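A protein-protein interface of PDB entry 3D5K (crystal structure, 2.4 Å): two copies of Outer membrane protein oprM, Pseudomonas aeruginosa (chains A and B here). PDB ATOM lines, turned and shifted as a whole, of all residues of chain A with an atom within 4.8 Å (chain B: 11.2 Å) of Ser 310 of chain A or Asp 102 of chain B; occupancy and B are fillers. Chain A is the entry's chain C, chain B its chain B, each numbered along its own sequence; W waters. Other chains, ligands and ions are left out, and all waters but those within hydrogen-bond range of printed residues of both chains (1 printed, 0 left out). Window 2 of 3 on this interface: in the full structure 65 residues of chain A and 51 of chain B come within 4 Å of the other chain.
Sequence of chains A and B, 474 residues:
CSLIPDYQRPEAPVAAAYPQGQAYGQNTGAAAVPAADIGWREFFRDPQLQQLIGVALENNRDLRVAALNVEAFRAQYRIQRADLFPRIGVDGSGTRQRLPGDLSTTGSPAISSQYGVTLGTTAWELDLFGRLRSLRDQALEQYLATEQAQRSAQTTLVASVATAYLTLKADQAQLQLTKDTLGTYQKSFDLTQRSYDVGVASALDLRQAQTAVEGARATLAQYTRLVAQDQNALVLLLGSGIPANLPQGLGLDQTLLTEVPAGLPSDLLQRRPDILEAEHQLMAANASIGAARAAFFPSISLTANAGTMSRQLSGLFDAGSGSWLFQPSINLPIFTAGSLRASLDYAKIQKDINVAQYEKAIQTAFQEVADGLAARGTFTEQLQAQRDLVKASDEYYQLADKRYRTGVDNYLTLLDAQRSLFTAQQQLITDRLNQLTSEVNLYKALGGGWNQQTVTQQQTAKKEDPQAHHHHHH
The backbone carbonyl oxygen of Asp 102 of chain B lies within hydrogen-bond range of the guanidinium group of Arg 311 of chain A (3.0 Å).
O of Pro 100 of chain B lies within hydrogen-bond range of OG of Ser 104 of chain B. The backbone carbonyl oxygen (O) of Ser 113 of chain A sits close to the guanidinium group (NH1) of Arg 311 of chain A. The backbone carbonyl oxygen (O) of Ser 310 of chain A lies within hydrogen-bond range of the backbone NH (N) of Tyr 115 of chain A, 2.7 Å away. OG of Ser 310 of chain A is in hydrogen-bond range of O of Gln 312 of chain A, at 2.8 Å. OG of Ser 310 of chain A lies within hydrogen-bond range of O of Gly 315 of chain A (3.2 Å).
Among the printed residues, pairs that only touch across the chains: Gln 114 of chain A with Leu 103 of chain B (3.8 Å), Met 309 of chain A with Pro 100 of chain B (3.4 Å), Met 309 of chain A with Leu 103 of chain B (3.7 Å), Ser 310 of chain A with Asp 102 of chain B (3.9 Å), Ser 310 of chain A with Leu 103 of chain B (3.6 Å) and Arg 311 of chain A with Leu 103 of chain B (3.3 Å).
Of the printed residues of chain B, Ser 310 of chain A touches Asp 102 (3.9 Å) and Leu 103 (3.6 Å). Asp 102 of chain B touches just these residues of chain A: Ser 310 and Arg 311. Of the printed residues of chain B, Met 309 of chain A touches Pro 100 (3.4 Å) and Leu 103 (3.7 Å). Arg 311 of chain A touches just these residues of chain B: Asp 102 and Leu 103. No residue of chain B comes within 4 Å of Gly 315 of chain A. Printed residues of chain A within 4 Å of Pro 100 of chain B: Met 309 (3.4 Å). Printed residues of chain A within 4 Å of Leu 103 of chain B: Gln 114, Met 309, Ser 310 and Arg 311. The nearest residue of chain B that does not touch Ser 310 of chain A is Pro 100 of chain B (5.0 Å). The nearest printed residue of chain A that does not touch Pro 100 of chain B is Ser 310 of chain A (5.0 Å).
Hydrophobic or aromatic side chains of chain B that line the printed part of chain A: Pro 100 and Leu 103. Hydrophobic or aromatic side chains of chain A within 4 Å of the printed part of chain B: Met 309. Among the printed residues, 7 pairs touch across the chains. Among the printed residues, no Asp or Glu carboxylate lies within 4 Å of a Lys or Arg side-chain nitrogen of the other chain.
No position is printed for both chains. Of the 7 pairs that touch across the chains among the printed residues, none has its exchanged pair printed and touching as well.
Water W1 lies within hydrogen-bond range of the side-chain carboxylate (OD1) of Asp 102 of chain B (3.0 Å) and the backbone carbonyl oxygen (O) of Met 309 of chain A (3.0 Å).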
ATOM      1  N   SER A 113       7.331 -26.928 -28.457  1.00  0.00           N
ATOM      2  CA  SER A 113       7.798 -26.945 -29.840  1.00  0.00           C
ATOM      3  C   SER A 113       9.168 -26.297 -29.980  1.00  0.00           C
ATOM      4  O   SER A 113       9.406 -25.217 -29.442  1.00  0.00           O
ATOM      5  CB  SER A 113       6.793 -26.247 -30.764  1.00  0.00           C
ATOM      6  OG  SER A 113       6.749 -24.851 -30.525  1.00  0.00           O
ATOM      7  N   GLN A 114      10.059 -26.965 -30.705  1.00  0.00           N
ATOM      8  CA  GLN A 114      11.402 -26.442 -30.955  1.00  0.00           C
ATOM      9  C   GLN A 114      11.906 -26.772 -32.359  1.00  0.00           C
ATOM     10  O   GLN A 114      11.570 -27.814 -32.929  1.00  0.00           O
ATOM     11  CB  GLN A 114      12.398 -26.916 -29.888  1.00  0.00           C
ATOM     12  CG  GLN A 114      12.440 -28.416 -29.671  1.00  0.00           C
ATOM     13  CD  GLN A 114      13.483 -28.822 -28.653  1.00  0.00           C
ATOM     14  OE1 GLN A 114      14.678 -28.592 -28.843  1.00  0.00           O
ATOM     15  NE2 GLN A 114      13.038 -29.435 -27.561  1.00  0.00           N
ATOM     16  N   TYR A 115      12.711 -25.861 -32.899  1.00  0.00           N
ATOM     17  CA  TYR A 115      13.271 -25.987 -34.237  1.00  0.00           C
ATOM     18  C   TYR A 115      14.787 -25.841 -34.163  1.00  0.00           C
ATOM     19  O   TYR A 115      15.330 -25.475 -33.119  1.00  0.00           O
ATOM     20  CB  TYR A 115      12.676 -24.925 -35.169  1.00  0.00           C
ATOM     21  CG  TYR A 115      11.163 -24.945 -35.253  1.00  0.00           C
ATOM     22  CD1 TYR A 115      10.387 -24.167 -34.396  1.00  0.00           C
ATOM     23  CD2 TYR A 115      10.508 -25.744 -36.190  1.00  0.00           C
ATOM     24  CE1 TYR A 115       8.997 -24.182 -34.469  1.00  0.00           C
ATOM     25  CE2 TYR A 115       9.114 -25.768 -36.272  1.00  0.00           C
ATOM     26  CZ  TYR A 115       8.366 -24.984 -35.409  1.00  0.00           C
ATOM     27  OH  TYR A 115       6.992 -25.002 -35.485  1.00  0.00           O
ATOM     28  N   THR A 308      21.916 -22.937 -34.929  1.00  0.00           N
ATOM     29  CA  THR A 308      20.868 -22.090 -34.384  1.00  0.00           C
ATOM     30  C   THR A 308      19.626 -22.898 -34.008  1.00  0.00           C
ATOM     31  O   THR A 308      19.163 -23.744 -34.775  1.00  0.00           O
ATOM     32  CB  THR A 308      20.521 -20.927 -35.356  1.00  0.00           C
ATOM     33  OG1 THR A 308      19.473 -20.126 -34.802  1.00  0.00           O
ATOM     34  CG2 THR A 308      20.104 -21.446 -36.732  1.00  0.00           C
ATOM     35  N   MET A 309      19.109 -22.639 -32.809  1.00  0.00           N
ATOM     36  CA  MET A 309      17.939 -23.345 -32.287  1.00  0.00           C
ATOM     37  C   MET A 309      16.948 -22.371 -31.663  1.00  0.00           C
ATOM     38  O   MET A 309      17.344 -21.401 -31.014  1.00  0.00           O
ATOM     39  CB  MET A 309      18.358 -24.391 -31.257  1.00  0.00           C
ATOM     40  CG  MET A 309      18.979 -25.650 -31.840  1.00  0.00           C
ATOM     41  SD  MET A 309      19.286 -26.895 -30.570  1.00  0.00           S
ATOM     42  CE  MET A 309      17.619 -27.469 -30.226  1.00  0.00           C
ATOM     43  N   SER A 310      15.660 -22.641 -31.857  1.00  0.00           N
ATOM     44  CA  SER A 310      14.605 -21.736 -31.417  1.00  0.00           C
ATOM     45  C   SER A 310      13.317 -22.478 -31.084  1.00  0.00           C
ATOM     46  O   SER A 310      13.103 -23.603 -31.533  1.00  0.00           O
ATOM     47  CB  SER A 310      14.334 -20.680 -32.493  1.00  0.00           C
ATOM     48  OG  SER A 310      13.333 -19.764 -32.085  1.00  0.00           O
ATOM     49  N   ARG A 311      12.445 -21.842 -30.359  1.00  0.00           N
ATOM     50  CA  ARG A 311      11.207 -22.444 -30.033  1.00  0.00           C
ATOM     51  C   ARG A 311      10.181 -22.158 -31.111  1.00  0.00           C
ATOM     52  O   ARG A 311       9.267 -22.928 -31.291  1.00  0.00           O
ATOM     53  CB  ARG A 311      10.801 -21.928 -28.687  1.00  0.00           C
ATOM     54  CG  ARG A 311       9.521 -22.399 -28.185  1.00  0.00           C
ATOM     55  CD  ARG A 311       9.575 -22.448 -26.712  1.00  0.00           C
ATOM     56  NE  ARG A 311      10.507 -23.467 -26.305  1.00  0.00           N
ATOM     57  CZ  ARG A 311      10.190 -24.728 -26.133  1.00  0.00           C
ATOM     58  NH1 ARG A 311       8.964 -25.128 -26.322  1.00  0.00           N
ATOM     59  NH2 ARG A 311      11.105 -25.580 -25.782  1.00  0.00           N
ATOM     60  N   GLN A 312      10.376 -21.074 -31.855  1.00  0.00           N
ATOM     61  CA  GLN A 312       9.551 -20.742 -33.019  1.00  0.00           C
ATOM     62  C   GLN A 312      10.408 -20.642 -34.284  1.00  0.00           C
ATOM     63  O   GLN A 312      11.564 -20.217 -34.228  1.00  0.00           O
ATOM     64  CB  GLN A 312       8.801 -19.426 -32.786  1.00  0.00           C
ATOM     65  CG  GLN A 312       7.690 -19.508 -31.742  1.00  0.00           C
ATOM     66  CD  GLN A 312       7.507 -18.213 -30.964  1.00  0.00           C
ATOM     67  OE1 GLN A 312       8.465 -17.475 -30.726  1.00  0.00           O
ATOM     68  NE2 GLN A 312       6.274 -17.939 -30.551  1.00  0.00           N
ATOM     69  N   GLY A 315      12.031 -17.258 -35.142  1.00  0.00           N
ATOM     70  CA  GLY A 315      13.055 -16.806 -34.205  1.00  0.00           C
ATOM     71  C   GLY A 315      14.371 -17.559 -34.287  1.00  0.00           C
ATOM     72  O   GLY A 315      15.184 -17.490 -33.360  1.00  0.00           O
ATOM     73  N   LEU A 316      14.589 -18.265 -35.397  1.00  0.00           N
ATOM     74  CA  LEU A 316      15.780 -19.102 -35.564  1.00  0.00           C
ATOM     75  C   LEU A 316      17.085 -18.311 -35.656  1.00  0.00           C
ATOM     76  O   LEU A 316      17.882 -18.343 -34.722  1.00  0.00           O
ATOM     77  CB  LEU A 316      15.625 -20.077 -36.743  1.00  0.00           C
ATOM     78  CG  LEU A 316      15.059 -21.462 -36.397  1.00  0.00           C
ATOM     79  CD1 LEU A 316      14.516 -22.150 -37.633  1.00  0.00           C
ATOM     80  CD2 LEU A 316      16.101 -22.342 -35.714  1.00  0.00           C
ATOM     81  N   ARG B  98      25.426 -25.782 -25.560  1.00  0.00           N
ATOM     82  CA  ARG B  98      24.893 -24.437 -25.396  1.00  0.00           C
ATOM     83  C   ARG B  98      23.438 -24.421 -25.864  1.00  0.00           C
ATOM     84  O   ARG B  98      23.117 -24.894 -26.960  1.00  0.00           O
ATOM     85  CB  ARG B  98      25.718 -23.407 -26.171  1.00  0.00           C
ATOM     86  CG  ARG B  98      25.311 -21.955 -25.909  1.00  0.00           C
ATOM     87  CD  ARG B  98      26.230 -20.960 -26.610  1.00  0.00           C
ATOM     88  NE  ARG B  98      26.018 -20.918 -28.060  1.00  0.00           N
ATOM     89  CZ  ARG B  98      26.872 -20.392 -28.937  1.00  0.00           C
ATOM     90  NH1 ARG B  98      28.021 -19.859 -28.528  1.00  0.00           N
ATOM     91  NH2 ARG B  98      26.583 -20.408 -30.232  1.00  0.00           N
ATOM     92  N   LEU B  99      22.565 -23.894 -25.013  1.00  0.00           N
ATOM     93  CA  LEU B  99      21.159 -23.729 -25.349  1.00  0.00           C
ATOM     94  C   LEU B  99      20.758 -22.271 -25.160  1.00  0.00           C
ATOM     95  O   LEU B  99      21.141 -21.652 -24.164  1.00  0.00           O
ATOM     96  CB  LEU B  99      20.283 -24.639 -24.480  1.00  0.00           C
ATOM     97  CG  LEU B  99      20.313 -26.146 -24.756  1.00  0.00           C
ATOM     98  CD1 LEU B  99      19.924 -26.929 -23.508  1.00  0.00           C
ATOM     99  CD2 LEU B  99      19.417 -26.517 -25.934  1.00  0.00           C
ATOM    100  N   PRO B 100      20.002 -21.710 -26.124  1.00  0.00           N
ATOM    101  CA  PRO B 100      19.446 -20.362 -25.978  1.00  0.00           C
ATOM    102  C   PRO B 100      18.456 -20.267 -24.814  1.00  0.00           C
ATOM    103  O   PRO B 100      17.995 -21.293 -24.309  1.00  0.00           O
ATOM    104  CB  PRO B 100      18.732 -20.127 -27.315  1.00  0.00           C
ATOM    105  CG  PRO B 100      18.482 -21.489 -27.863  1.00  0.00           C
ATOM    106  CD  PRO B 100      19.643 -22.311 -27.422  1.00  0.00           C
ATOM    107  N   GLY B 101      18.135 -19.042 -24.405  1.00  0.00           N
ATOM    108  CA  GLY B 101      17.261 -18.797 -23.258  1.00  0.00           C
ATOM    109  C   GLY B 101      15.864 -19.385 -23.339  1.00  0.00           C
ATOM    110  O   GLY B 101      15.313 -19.828 -22.330  1.00  0.00           O
ATOM    111  N   ASP B 102      15.321 -19.454 -24.528  1.00  0.00           N
ATOM    112  CA  ASP B 102      13.961 -19.913 -24.703  1.00  0.00           C
ATOM    113  C   ASP B 102      13.853 -21.409 -24.837  1.00  0.00           C
ATOM    114  O   ASP B 102      12.787 -21.916 -25.053  1.00  0.00           O
ATOM    115  CB  ASP B 102      13.323 -19.259 -25.914  1.00  0.00           C
ATOM    116  CG  ASP B 102      14.195 -19.300 -27.089  1.00  0.00           C
ATOM    117  OD1 ASP B 102      15.376 -19.071 -26.907  1.00  0.00           O
ATOM    118  OD2 ASP B 102      13.734 -19.580 -28.190  1.00  0.00           O
ATOM    119  N   LEU B 103      14.913 -22.132 -24.680  1.00  0.00           N
ATOM    120  CA  LEU B 103      14.899 -23.570 -24.837  1.00  0.00           C
ATOM    121  C   LEU B 103      15.518 -24.197 -23.639  1.00  0.00           C
ATOM    122  O   LEU B 103      15.610 -25.381 -23.559  1.00  0.00           O
ATOM    123  CB  LEU B 103      15.734 -23.952 -26.040  1.00  0.00           C
ATOM    124  CG  LEU B 103      15.169 -24.532 -27.315  1.00  0.00           C
ATOM    125  CD1 LEU B 103      13.707 -24.438 -27.389  1.00  0.00           C
ATOM    126  CD2 LEU B 103      15.820 -23.959 -28.530  1.00  0.00           C
ATOM    127  N   SER B 104      16.081 -23.352 -22.777  1.00  0.00           N
ATOM    128  CA  SER B 104      16.916 -23.783 -21.673  1.00  0.00           C
ATOM    129  C   SER B 104      15.898 -23.824 -20.525  1.00  0.00           C
ATOM    130  O   SER B 104      14.696 -23.732 -20.772  1.00  0.00           O
ATOM    131  CB  SER B 104      17.911 -22.713 -21.266  1.00  0.00           C
ATOM    132  OG  SER B 104      17.269 -21.469 -21.052  1.00  0.00           O
ATOM    133  N   THR B 105      16.361 -23.936 -19.283  1.00  0.00           N
ATOM    134  CA  THR B 105      15.388 -23.828 -18.224  1.00  0.00           C
ATOM    135  C   THR B 105      15.154 -22.603 -17.357  1.00  0.00           C
ATOM    136  O   THR B 105      14.166 -22.431 -16.684  1.00  0.00           O
ATOM    137  CB  THR B 105      15.745 -25.074 -17.353  1.00  0.00           C
ATOM    138  OG1 THR B 105      17.139 -25.375 -17.487  1.00  0.00           O
ATOM    139  CG2 THR B 105      14.988 -26.245 -17.842  1.00  0.00           C
ATOM    140  N   THR B 106      16.037 -21.675 -17.591  1.00  0.00           N
ATOM    141  CA  THR B 106      16.735 -20.825 -16.641  1.00  0.00           C
ATOM    142  C   THR B 106      16.191 -19.541 -17.255  1.00  0.00           C
ATOM    143  O   THR B 106      16.125 -18.497 -16.630  1.00  0.00           O
ATOM    144  CB  THR B 106      18.246 -20.698 -16.434  1.00  0.00           C
ATOM    145  OG1 THR B 106      18.893 -20.620 -17.687  1.00  0.00           O
ATOM    146  CG2 THR B 106      18.800 -21.913 -15.715  1.00  0.00           C
ATOM    147  N   GLY B 107      15.801 -19.675 -18.490  1.00  0.00           N
ATOM    148  CA  GLY B 107      15.260 -18.577 -19.288  1.00  0.00           C
ATOM    149  C   GLY B 107      16.347 -17.759 -19.962  1.00  0.00           C
ATOM    150  O   GLY B 107      16.060 -16.890 -20.789  1.00  0.00           O
ATOM    151  N   SER B 108      17.598 -18.046 -19.601  1.00  0.00           N
ATOM    152  CA  SER B 108      18.768 -17.358 -20.145  1.00  0.00           C
ATOM    153  C   SER B 108      19.771 -18.367 -20.718  1.00  0.00           C
ATOM    154  O   SER B 108      19.824 -19.512 -20.252  1.00  0.00           O
ATOM    155  CB  SER B 108      19.429 -16.499 -19.060  1.00  0.00           C
ATOM    156  OG  SER B 108      19.748 -17.270 -17.914  1.00  0.00           O
ATOM    157  N   PRO B 109      20.549 -17.956 -21.746  1.00  0.00           N
ATOM    158  CA  PRO B 109      21.593 -18.802 -22.339  1.00  0.00           C
ATOM    159  C   PRO B 109      22.450 -19.522 -21.297  1.00  0.00           C
ATOM    160  O   PRO B 109      22.899 -18.909 -20.323  1.00  0.00           O
ATOM    161  CB  PRO B 109      22.434 -17.802 -23.130  1.00  0.00           C
ATOM    162  CG  PRO B 109      21.444 -16.790 -23.577  1.00  0.00           C
ATOM    163  CD  PRO B 109      20.457 -16.657 -22.439  1.00  0.00           C
ATOM    164  N   ALA B 110      22.663 -20.817 -21.514  1.00  0.00           N
ATOM    165  CA  ALA B 110      23.356 -21.667 -20.556  1.00  0.00           C
ATOM    166  C   ALA B 110      24.154 -22.773 -21.243  1.00  0.00           C
ATOM    167  O   ALA B 110      23.879 -23.136 -22.389  1.00  0.00           O
ATOM    168  CB  ALA B 110      22.355 -22.272 -19.573  1.00  0.00           C
HETATM  169  O   HOH W   1      16.212 -18.939 -29.735  1.00  0.00           O
